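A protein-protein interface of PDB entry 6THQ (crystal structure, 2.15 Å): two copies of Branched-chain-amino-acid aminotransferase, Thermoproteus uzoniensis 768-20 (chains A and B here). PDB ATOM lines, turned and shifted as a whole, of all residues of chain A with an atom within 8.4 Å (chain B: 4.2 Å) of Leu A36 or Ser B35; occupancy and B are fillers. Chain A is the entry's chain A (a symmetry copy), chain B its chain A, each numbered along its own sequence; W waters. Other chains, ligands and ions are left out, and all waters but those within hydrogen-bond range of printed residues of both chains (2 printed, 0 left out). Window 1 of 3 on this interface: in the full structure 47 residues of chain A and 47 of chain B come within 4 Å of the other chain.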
ATOM      1  N   VAL A  29      -5.211  -9.331 -26.802  1.00  0.00           N
ATOM      2  CA  VAL A  29      -4.323  -9.717 -25.659  1.00  0.00           C
ATOM      3  C   VAL A  29      -3.157 -10.571 -26.186  1.00  0.00           C
ATOM      4  O   VAL A  29      -3.311 -11.336 -27.155  1.00  0.00           O
ATOM      5  CB  VAL A  29      -5.127 -10.446 -24.552  1.00  0.00           C
ATOM      6  CG1 VAL A  29      -5.829 -11.704 -25.119  1.00  0.00           C
ATOM      7  CG2 VAL A  29      -4.282 -10.715 -23.326  1.00  0.00           C
ATOM      8  N   THR A  30      -1.986 -10.376 -25.593  1.00  0.00           N
ATOM      9  CA  THR A  30      -0.806 -11.144 -25.965  1.00  0.00           C
ATOM     10  C   THR A  30      -1.112 -12.673 -25.890  1.00  0.00           C
ATOM     11  O   THR A  30      -1.716 -13.169 -24.934  1.00  0.00           O
ATOM     12  CB  THR A  30       0.374 -10.835 -25.040  1.00  0.00           C
ATOM     13  OG1 THR A  30       1.361 -11.862 -25.213  1.00  0.00           O
ATOM     14  CG2 THR A  30      -0.019 -10.860 -23.546  1.00  0.00           C
ATOM     15  N   VAL A  31      -0.678 -13.407 -26.914  1.00  0.00           N
ATOM     16  CA  VAL A  31      -0.820 -14.825 -26.965  1.00  0.00           C
ATOM     17  C   VAL A  31      -0.016 -15.516 -25.871  1.00  0.00           C
ATOM     18  O   VAL A  31      -0.074 -16.741 -25.741  1.00  0.00           O
ATOM     19  CB  VAL A  31      -0.452 -15.397 -28.342  1.00  0.00           C
ATOM     20  CG1 VAL A  31      -1.415 -14.825 -29.406  1.00  0.00           C
ATOM     21  CG2 VAL A  31       1.021 -15.133 -28.632  1.00  0.00           C
ATOM     22  N   LEU A  32       0.723 -14.762 -25.077  1.00  0.00           N
ATOM     23  CA  LEU A  32       1.495 -15.368 -23.989  1.00  0.00           C
ATOM     24  C   LEU A  32       0.811 -15.159 -22.672  1.00  0.00           C
ATOM     25  O   LEU A  32       1.401 -15.420 -21.625  1.00  0.00           O
ATOM     26  CB  LEU A  32       2.898 -14.742 -23.895  1.00  0.00           C
ATOM     27  CG  LEU A  32       3.868 -15.182 -24.998  1.00  0.00           C
ATOM     28  CD1 LEU A  32       5.222 -14.549 -24.775  1.00  0.00           C
ATOM     29  CD2 LEU A  32       4.024 -16.696 -25.147  1.00  0.00           C
ATOM     30  N   SER A  33      -0.423 -14.651 -22.710  1.00  0.00           N
ATOM     31  CA  SER A  33      -1.143 -14.397 -21.493  1.00  0.00           C
ATOM     32  C   SER A  33      -1.474 -15.709 -20.805  1.00  0.00           C
ATOM     33  O   SER A  33      -1.951 -16.640 -21.466  1.00  0.00           O
ATOM     34  CB  SER A  33      -2.449 -13.663 -21.837  1.00  0.00           C
ATOM     35  OG  SER A  33      -3.252 -13.626 -20.692  1.00  0.00           O
ATOM     36  N   PRO A  34      -1.248 -15.775 -19.496  1.00  0.00           N
ATOM     37  CA  PRO A  34      -1.684 -16.950 -18.733  1.00  0.00           C
ATOM     38  C   PRO A  34      -3.224 -17.123 -18.803  1.00  0.00           C
ATOM     39  O   PRO A  34      -3.708 -18.234 -18.591  1.00  0.00           O
ATOM     40  CB  PRO A  34      -1.275 -16.653 -17.267  1.00  0.00           C
ATOM     41  CG  PRO A  34      -1.086 -15.152 -17.214  1.00  0.00           C
ATOM     42  CD  PRO A  34      -0.656 -14.731 -18.637  1.00  0.00           C
ATOM     43  N   SER A  35      -3.981 -16.077 -19.157  1.00  0.00           N
ATOM     44  CA  SER A  35      -5.408 -16.247 -19.392  1.00  0.00           C
ATOM     45  C   SER A  35      -5.648 -17.002 -20.662  1.00  0.00           C
ATOM     46  O   SER A  35      -6.627 -17.765 -20.763  1.00  0.00           O
ATOM     47  CB  SER A  35      -6.177 -14.915 -19.402  1.00  0.00           C
ATOM     48  OG  SER A  35      -5.964 -14.261 -18.159  1.00  0.00           O
ATOM     49  N   LEU A  36      -4.773 -16.805 -21.654  1.00  0.00           N
ATOM     50  CA  LEU A  36      -4.979 -17.535 -22.897  1.00  0.00           C
ATOM     51  C   LEU A  36      -4.393 -18.957 -22.772  1.00  0.00           C
ATOM     52  O   LEU A  36      -4.920 -19.931 -23.335  1.00  0.00           O
ATOM     53  CB  LEU A  36      -4.352 -16.773 -24.068  1.00  0.00           C
ATOM     54  CG  LEU A  36      -4.506 -17.550 -25.367  1.00  0.00           C
ATOM     55  CD1 LEU A  36      -5.919 -17.457 -25.904  1.00  0.00           C
ATOM     56  CD2 LEU A  36      -3.484 -17.235 -26.419  1.00  0.00           C
ATOM     57  N   ASN A  37      -3.304 -19.080 -22.023  1.00  0.00           N
ATOM     58  CA  ASN A  37      -2.533 -20.335 -22.012  1.00  0.00           C
ATOM     59  C   ASN A  37      -3.112 -21.326 -20.991  1.00  0.00           C
ATOM     60  O   ASN A  37      -2.987 -22.542 -21.180  1.00  0.00           O
ATOM     61  CB  ASN A  37      -1.055 -20.092 -21.706  1.00  0.00           C
ATOM     62  CG  ASN A  37      -0.249 -19.684 -22.957  1.00  0.00           C
ATOM     63  OD1 ASN A  37       0.565 -20.486 -23.511  1.00  0.00           O
ATOM     64  ND2 ASN A  37      -0.421 -18.405 -23.387  1.00  0.00           N
ATOM     65  N   TYR A  38      -3.737 -20.806 -19.926  1.00  0.00           N
ATOM     66  CA  TYR A  38      -4.085 -21.618 -18.755  1.00  0.00           C
ATOM     67  C   TYR A  38      -5.546 -21.473 -18.285  1.00  0.00           C
ATOM     68  O   TYR A  38      -5.852 -21.949 -17.216  1.00  0.00           O
ATOM     69  CB  TYR A  38      -3.191 -21.301 -17.584  1.00  0.00           C
ATOM     70  CG  TYR A  38      -1.737 -21.367 -17.901  1.00  0.00           C
ATOM     71  CD1 TYR A  38      -1.206 -22.441 -18.642  1.00  0.00           C
ATOM     72  CD2 TYR A  38      -0.863 -20.355 -17.463  1.00  0.00           C
ATOM     73  CE1 TYR A  38       0.171 -22.498 -18.917  1.00  0.00           C
ATOM     74  CE2 TYR A  38       0.501 -20.386 -17.776  1.00  0.00           C
ATOM     75  CZ  TYR A  38       1.012 -21.454 -18.478  1.00  0.00           C
ATOM     76  OH  TYR A  38       2.346 -21.480 -18.775  1.00  0.00           O
ATOM     77  N   GLY A  39      -6.426 -20.829 -19.081  1.00  0.00           N
ATOM     78  CA  GLY A  39      -7.866 -20.741 -18.795  1.00  0.00           C
ATOM     79  C   GLY A  39      -8.121 -19.938 -17.578  1.00  0.00           C
ATOM     80  O   GLY A  39      -9.094 -20.188 -16.877  1.00  0.00           O
ATOM     81  N   PHE A  40      -7.239 -18.970 -17.277  1.00  0.00           N
ATOM     82  CA  PHE A  40      -7.387 -18.231 -16.023  1.00  0.00           C
ATOM     83  C   PHE A  40      -7.991 -16.839 -16.256  1.00  0.00           C
ATOM     84  O   PHE A  40      -7.286 -15.861 -16.369  1.00  0.00           O
ATOM     85  CB  PHE A  40      -6.043 -18.163 -15.317  1.00  0.00           C
ATOM     86  CG  PHE A  40      -6.094 -17.459 -14.010  1.00  0.00           C
ATOM     87  CD1 PHE A  40      -6.620 -18.103 -12.885  1.00  0.00           C
ATOM     88  CD2 PHE A  40      -5.575 -16.129 -13.859  1.00  0.00           C
ATOM     89  CE1 PHE A  40      -6.623 -17.462 -11.633  1.00  0.00           C
ATOM     90  CE2 PHE A  40      -5.573 -15.523 -12.609  1.00  0.00           C
ATOM     91  CZ  PHE A  40      -6.099 -16.172 -11.501  1.00  0.00           C
ATOM     92  N   GLY A  41      -9.311 -16.806 -16.403  1.00  0.00           N
ATOM     93  CA  GLY A  41     -10.094 -15.572 -16.380  1.00  0.00           C
ATOM     94  C   GLY A  41     -11.552 -15.784 -16.035  1.00  0.00           C
ATOM     95  O   GLY A  41     -11.965 -16.895 -15.769  1.00  0.00           O
ATOM     96  N   TYR A 109      -9.241 -10.742 -17.653  1.00  0.00           N
ATOM     97  CA  TYR A 109      -8.093 -11.557 -18.002  1.00  0.00           C
ATOM     98  C   TYR A 109      -6.821 -10.836 -17.678  1.00  0.00           C
ATOM     99  O   TYR A 109      -6.827  -9.639 -17.351  1.00  0.00           O
ATOM    100  CB  TYR A 109      -8.114 -11.887 -19.487  1.00  0.00           C
ATOM    101  CG  TYR A 109      -8.127 -10.662 -20.295  1.00  0.00           C
ATOM    102  CD1 TYR A 109      -9.341  -9.986 -20.541  1.00  0.00           C
ATOM    103  CD2 TYR A 109      -6.953 -10.110 -20.740  1.00  0.00           C
ATOM    104  CE1 TYR A 109      -9.351  -8.819 -21.282  1.00  0.00           C
ATOM    105  CE2 TYR A 109      -6.939  -8.939 -21.455  1.00  0.00           C
ATOM    106  CZ  TYR A 109      -8.136  -8.295 -21.709  1.00  0.00           C
ATOM    107  OH  TYR A 109      -8.126  -7.140 -22.409  1.00  0.00           O
ATOM    108  N   ILE A 110      -5.718 -11.581 -17.713  1.00  0.00           N
ATOM    109  CA  ILE A 110      -4.417 -11.012 -17.461  1.00  0.00           C
ATOM    110  C   ILE A 110      -3.762 -10.562 -18.776  1.00  0.00           C
ATOM    111  O   ILE A 110      -3.633 -11.355 -19.707  1.00  0.00           O
ATOM    112  CB  ILE A 110      -3.584 -11.995 -16.671  1.00  0.00           C
ATOM    113  CG1 ILE A 110      -4.144 -11.865 -15.239  1.00  0.00           C
ATOM    114  CG2 ILE A 110      -2.130 -11.533 -16.704  1.00  0.00           C
ATOM    115  CD1 ILE A 110      -3.705 -12.987 -14.364  1.00  0.00           C
ATOM    116  N   SER A 111      -3.366  -9.295 -18.862  1.00  0.00           N
ATOM    117  CA  SER A 111      -2.844  -8.796 -20.160  1.00  0.00           C
ATOM    118  C   SER A 111      -1.343  -8.846 -20.273  1.00  0.00           C
ATOM    119  O   SER A 111      -0.860  -8.734 -21.380  1.00  0.00           O
ATOM    120  CB  SER A 111      -3.355  -7.389 -20.527  1.00  0.00           C
ATOM    121  OG  SER A 111      -3.083  -6.584 -19.430  1.00  0.00           O
ATOM    122  N   LYS A 112      -0.650  -9.056 -19.150  1.00  0.00           N
ATOM    123  CA  LYS A 112       0.800  -9.322 -19.094  1.00  0.00           C
ATOM    124  C   LYS A 112       1.172 -10.728 -19.697  1.00  0.00           C
ATOM    125  O   LYS A 112       0.500 -11.727 -19.461  1.00  0.00           O
ATOM    126  CB  LYS A 112       1.232  -9.130 -17.605  1.00  0.00           C
ATOM    127  CG  LYS A 112       2.618  -9.641 -17.155  1.00  0.00           C
ATOM    128  CD  LYS A 112       2.949  -9.166 -15.746  1.00  0.00           C
ATOM    129  CE  LYS A 112       4.428  -9.289 -15.393  1.00  0.00           C
ATOM    130  NZ  LYS A 112       4.650 -10.693 -14.961  1.00  0.00           N
ATOM    131  N   GLN A 114       2.999 -14.217 -19.528  1.00  0.00           N
ATOM    132  CA  GLN A 114       3.576 -14.950 -18.359  1.00  0.00           C
ATOM    133  C   GLN A 114       3.382 -16.435 -18.501  1.00  0.00           C
ATOM    134  O   GLN A 114       2.272 -16.905 -18.615  1.00  0.00           O
ATOM    135  CB  GLN A 114       3.047 -14.477 -16.999  1.00  0.00           C
ATOM    136  CG  GLN A 114       3.637 -15.227 -15.827  1.00  0.00           C
ATOM    137  CD  GLN A 114       3.152 -14.673 -14.487  1.00  0.00           C
ATOM    138  OE1 GLN A 114       3.217 -13.479 -14.249  1.00  0.00           O
ATOM    139  NE2 GLN A 114       2.663 -15.535 -13.610  1.00  0.00           N
ATOM    140  N   THR A 164     -13.257 -18.940 -17.326  1.00  0.00           N
ATOM    141  CA  THR A 164     -13.045 -19.300 -18.718  1.00  0.00           C
ATOM    142  C   THR A 164     -12.581 -20.734 -18.937  1.00  0.00           C
ATOM    143  O   THR A 164     -13.112 -21.421 -19.785  1.00  0.00           O
ATOM    144  CB  THR A 164     -11.983 -18.355 -19.303  1.00  0.00           C
ATOM    145  OG1 THR A 164     -10.828 -18.444 -18.477  1.00  0.00           O
ATOM    146  CG2 THR A 164     -12.494 -16.862 -19.337  1.00  0.00           C
ATOM    147  N   GLY A 165     -11.580 -21.186 -18.192  1.00  0.00           N
ATOM    148  CA  GLY A 165     -10.999 -22.492 -18.484  1.00  0.00           C
ATOM    149  C   GLY A 165     -12.016 -23.614 -18.284  1.00  0.00           C
ATOM    150  O   GLY A 165     -11.923 -24.600 -18.976  1.00  0.00           O
ATOM    151  N   LEU A 168     -14.140 -25.374 -21.471  1.00  0.00           N
ATOM    152  CA  LEU A 168     -13.705 -26.473 -22.345  1.00  0.00           C
ATOM    153  C   LEU A 168     -14.657 -27.670 -22.142  1.00  0.00           C
ATOM    154  O   LEU A 168     -15.029 -28.381 -23.087  1.00  0.00           O
ATOM    155  CB  LEU A 168     -12.242 -26.848 -22.024  1.00  0.00           C
ATOM    156  CG  LEU A 168     -11.620 -28.018 -22.779  1.00  0.00           C
ATOM    157  CD1 LEU A 168     -11.667 -27.860 -24.294  1.00  0.00           C
ATOM    158  CD2 LEU A 168     -10.174 -28.189 -22.297  1.00  0.00           C
ATOM    159  N   ILE A 171     -17.764 -26.794 -24.041  1.00  0.00           N
ATOM    160  CA  ILE A 171     -17.464 -27.077 -25.451  1.00  0.00           C
ATOM    161  C   ILE A 171     -17.566 -28.545 -25.832  1.00  0.00           C
ATOM    162  O   ILE A 171     -18.245 -28.868 -26.817  1.00  0.00           O
ATOM    163  CB  ILE A 171     -16.157 -26.440 -25.896  1.00  0.00           C
ATOM    164  CG1 ILE A 171     -16.435 -24.947 -26.051  1.00  0.00           C
ATOM    165  CG2 ILE A 171     -15.772 -26.993 -27.251  1.00  0.00           C
ATOM    166  CD1 ILE A 171     -15.188 -24.109 -26.170  1.00  0.00           C
ATOM    167  N   SER B  33     -12.109 -14.039 -28.483  1.00  0.00           N
ATOM    168  CA  SER B  33     -11.800 -15.351 -28.981  1.00  0.00           C
ATOM    169  C   SER B  33     -12.388 -16.405 -28.060  1.00  0.00           C
ATOM    170  O   SER B  33     -12.232 -16.300 -26.836  1.00  0.00           O
ATOM    171  CB  SER B  33     -10.272 -15.515 -29.024  1.00  0.00           C
ATOM    172  OG  SER B  33      -9.976 -16.858 -29.282  1.00  0.00           O
ATOM    173  N   PRO B  34     -13.032 -17.416 -28.636  1.00  0.00           N
ATOM    174  CA  PRO B  34     -13.493 -18.551 -27.828  1.00  0.00           C
ATOM    175  C   PRO B  34     -12.301 -19.274 -27.148  1.00  0.00           C
ATOM    176  O   PRO B  34     -12.511 -19.952 -26.143  1.00  0.00           O
ATOM    177  CB  PRO B  34     -14.163 -19.518 -28.837  1.00  0.00           C
ATOM    178  CG  PRO B  34     -13.610 -19.113 -30.187  1.00  0.00           C
ATOM    179  CD  PRO B  34     -13.292 -17.605 -30.076  1.00  0.00           C
ATOM    180  N   SER B  35     -11.066 -19.090 -27.631  1.00  0.00           N
ATOM    181  CA  SER B  35      -9.911 -19.619 -26.919  1.00  0.00           C
ATOM    182  C   SER B  35      -9.663 -18.844 -25.663  1.00  0.00           C
ATOM    183  O   SER B  35      -9.201 -19.413 -24.656  1.00  0.00           O
ATOM    184  CB  SER B  35      -8.641 -19.662 -27.787  1.00  0.00           C
ATOM    185  OG  SER B  35      -8.907 -20.451 -28.938  1.00  0.00           O
ATOM    186  N   LEU B  36      -9.955 -17.540 -25.693  1.00  0.00           N
ATOM    187  CA  LEU B  36      -9.732 -16.766 -24.480  1.00  0.00           C
ATOM    188  C   LEU B  36     -10.934 -16.930 -23.526  1.00  0.00           C
ATOM    189  O   LEU B  36     -10.790 -16.942 -22.293  1.00  0.00           O
ATOM    190  CB  LEU B  36      -9.492 -15.294 -24.829  1.00  0.00           C
ATOM    191  CG  LEU B  36      -9.315 -14.459 -23.569  1.00  0.00           C
ATOM    192  CD1 LEU B  36      -7.945 -14.665 -22.955  1.00  0.00           C
ATOM    193  CD2 LEU B  36      -9.649 -13.004 -23.720  1.00  0.00           C
ATOM    194  N   ASN B  37     -12.124 -17.066 -24.098  1.00  0.00           N
ATOM    195  CA  ASN B  37     -13.358 -17.005 -23.298  1.00  0.00           C
ATOM    196  C   ASN B  37     -13.699 -18.382 -22.707  1.00  0.00           C
ATOM    197  O   ASN B  37     -14.324 -18.454 -21.643  1.00  0.00           O
ATOM    198  CB  ASN B  37     -14.543 -16.493 -24.116  1.00  0.00           C
ATOM    199  CG  ASN B  37     -14.592 -14.953 -24.192  1.00  0.00           C
ATOM    200  OD1 ASN B  37     -15.459 -14.286 -23.545  1.00  0.00           O
ATOM    201  ND2 ASN B  37     -13.696 -14.367 -25.030  1.00  0.00           N
ATOM    202  N   GLY B  39     -11.391 -21.469 -22.856  1.00  0.00           N
ATOM    203  CA  GLY B  39     -10.271 -22.382 -22.580  1.00  0.00           C
ATOM    204  C   GLY B  39     -10.076 -23.338 -23.693  1.00  0.00           C
ATOM    205  O   GLY B  39      -9.634 -24.458 -23.463  1.00  0.00           O
ATOM    206  N   PHE B  40     -10.425 -22.936 -24.926  1.00  0.00           N
ATOM    207  CA  PHE B  40     -10.360 -23.887 -26.036  1.00  0.00           C
ATOM    208  C   PHE B  40      -9.123 -23.648 -26.912  1.00  0.00           C
ATOM    209  O   PHE B  40      -9.188 -22.979 -27.920  1.00  0.00           O
ATOM    210  CB  PHE B  40     -11.651 -23.820 -26.834  1.00  0.00           C
ATOM    211  CG  PHE B  40     -11.699 -24.777 -27.968  1.00  0.00           C
ATOM    212  CD1 PHE B  40     -11.950 -26.133 -27.733  1.00  0.00           C
ATOM    213  CD2 PHE B  40     -11.530 -24.337 -29.325  1.00  0.00           C
ATOM    214  CE1 PHE B  40     -12.049 -27.037 -28.807  1.00  0.00           C
ATOM    215  CE2 PHE B  40     -11.650 -25.244 -30.369  1.00  0.00           C
ATOM    216  CZ  PHE B  40     -11.897 -26.587 -30.122  1.00  0.00           C
ATOM    217  N   VAL B 107       1.494 -22.062 -28.960  1.00  0.00           N
ATOM    218  CA  VAL B 107       0.138 -22.066 -28.511  1.00  0.00           C
ATOM    219  C   VAL B 107      -0.767 -22.013 -29.721  1.00  0.00           C
ATOM    220  O   VAL B 107      -0.548 -21.209 -30.595  1.00  0.00           O
ATOM    221  CB  VAL B 107      -0.119 -20.924 -27.512  1.00  0.00           C
ATOM    222  CG1 VAL B 107       0.389 -19.592 -28.021  1.00  0.00           C
ATOM    223  CG2 VAL B 107      -1.623 -20.845 -27.129  1.00  0.00           C
ATOM    224  N   TYR B 109      -4.714 -21.612 -31.048  1.00  0.00           N
ATOM    225  CA  TYR B 109      -5.925 -20.960 -30.588  1.00  0.00           C
ATOM    226  C   TYR B 109      -6.718 -20.449 -31.751  1.00  0.00           C
ATOM    227  O   TYR B 109      -6.245 -20.441 -32.897  1.00  0.00           O
ATOM    228  CB  TYR B 109      -5.581 -19.798 -29.670  1.00  0.00           C
ATOM    229  CG  TYR B 109      -4.716 -18.829 -30.353  1.00  0.00           C
ATOM    230  CD1 TYR B 109      -3.323 -19.044 -30.422  1.00  0.00           C
ATOM    231  CD2 TYR B 109      -5.259 -17.756 -31.014  1.00  0.00           C
ATOM    232  CE1 TYR B 109      -2.510 -18.145 -31.085  1.00  0.00           C
ATOM    233  CE2 TYR B 109      -4.472 -16.867 -31.701  1.00  0.00           C
ATOM    234  CZ  TYR B 109      -3.107 -17.074 -31.743  1.00  0.00           C
ATOM    235  OH  TYR B 109      -2.329 -16.203 -32.422  1.00  0.00           O
ATOM    236  N   ILE B 110      -7.962 -20.066 -31.469  1.00  0.00           N
ATOM    237  CA  ILE B 110      -8.829 -19.516 -32.481  1.00  0.00           C
ATOM    238  C   ILE B 110      -8.714 -17.984 -32.515  1.00  0.00           C
ATOM    239  O   ILE B 110      -8.896 -17.327 -31.492  1.00  0.00           O
ATOM    240  CB  ILE B 110     -10.238 -20.017 -32.262  1.00  0.00           C
ATOM    241  CG1 ILE B 110     -10.189 -21.463 -32.800  1.00  0.00           C
ATOM    242  CG2 ILE B 110     -11.187 -19.178 -33.114  1.00  0.00           C
ATOM    243  CD1 ILE B 110     -11.373 -22.258 -32.371  1.00  0.00           C
ATOM    244  N   THR B 164      -5.502 -25.784 -22.960  1.00  0.00           N
ATOM    245  CA  THR B 164      -5.392 -24.595 -22.132  1.00  0.00           C
ATOM    246  C   THR B 164      -6.388 -24.531 -20.982  1.00  0.00           C
ATOM    247  O   THR B 164      -6.008 -24.236 -19.867  1.00  0.00           O
ATOM    248  CB  THR B 164      -5.609 -23.364 -23.028  1.00  0.00           C
ATOM    249  OG1 THR B 164      -6.861 -23.527 -23.683  1.00  0.00           O
ATOM    250  CG2 THR B 164      -4.464 -23.224 -24.104  1.00  0.00           C
HETATM  251  O   HOH W   1      -9.148 -16.903 -20.333  1.00  0.00           O
HETATM  252  O   HOH W   2      -6.878 -20.783 -24.741  1.00  0.00           O
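The backbone carbonyl oxygen (O) of Ser B33 is in hydrogen-bond range of the side-chain amide nitrogen (ND2) of Asn B37 (3.0 Å). The backbone carbonyl oxygen (O) of Phe B40 sits at hydrogen-bond distance from the side-chain hydroxyl (OG) of Ser B35, 2.7 Å away. The backbone carbonyl oxygen (O) of Gly B39 is in hydrogen-bond range of the side-chain hydroxyl (OG1) of Thr B164, 2.9 Å away. The side-chain amide nitrogen of Asn A37 lies within hydrogen-bond range of the backbone carbonyl oxygen of Ser A33 (3.0 Å). O of Phe A40 sits at hydrogen-bond distance from OG of Ser A35 (2.7 Å). OG1 of Thr A164 is in hydrogen-bond range of O of Gly A39 (2.9 Å).
Water W2 lies within hydrogen-bond range of the backbone carbonyl oxygen (O) of Leu A36 (2.6 Å), the backbone carbonyl oxygen (O) of Ser B35 (2.7 Å) and the side-chain hydroxyl (OG1) of Thr B164 (2.9 Å). Water W1 lies within hydrogen-bond range of the backbone carbonyl oxygen (O) of Leu B36 (2.6 Å), the backbone carbonyl oxygen (O) of Ser A35 (2.7 Å) and the side-chain hydroxyl (OG1) of Thr A164 (2.9 Å).
Printed residues of chain A that touch a printed residue of chain B: Val A31, Ser A35, Leu A36, Asn A37, Tyr A38, Gly A39, Thr A164, Leu A168 and Ile A171. Hydrophobic or aromatic side chains of chain A within 4 Å of the printed part of chain B: Val A31, Leu A36, Leu A168 and Ile A171. Among the printed residues, 14 pairs touch across the chains.
Ser A35 touches Leu B36, and with the chains exchanged Leu A36 touches Ser B35. Leu A36 touches Thr B164, and with the chains exchanged Thr A164 touches Leu B36. Asn A37 touches Thr B164, and with the chains exchanged Thr A164 touches Asn B37. Gly A39 touches Thr B164, and with the chains exchanged Thr A164 touches Gly B39. 10 positions are printed for both chains.
Among the printed residues, pairs that only touch across the chains: Val A31 with Val B107 (3.7 Å), Val A31 with Tyr B109 (3.4 Å), Ser A35 with Leu B36 (3.98 Å), Leu A36 with Ser B35 (3.98 Å), Leu A36 with Thr B164 (3.4 Å), Asn A37 with Thr B164 (3.3 Å), Tyr A38 with Thr B164 (3.2 Å), Gly A39 with Thr B164 (3.5 Å), Thr A164 with Leu B36 (3.4 Å), Thr A164 with Asn B37 (3.3 Å), Thr A164 with Gly B39 (3.5 Å), Leu A168 with Gly B39 (3.8 Å), Leu A168 with Phe B40 (3.9 Å) and Ile A171 with Phe B40 (3.6 Å).
Pro B34 touches none of the printed residues of chain A. Of the printed residues of chain A, Val B107 touches Val A31 (3.7 Å). Printed residues of chain A within 4 Å of Leu B36: Ser A35 and Thr A164. The nearest residue of chain A that does not touch Ser B35 is Ser A35 (4.9 Å). The nearest printed residue of chain B that does not touch Asn A37 is Val B107 (4.1 Å).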
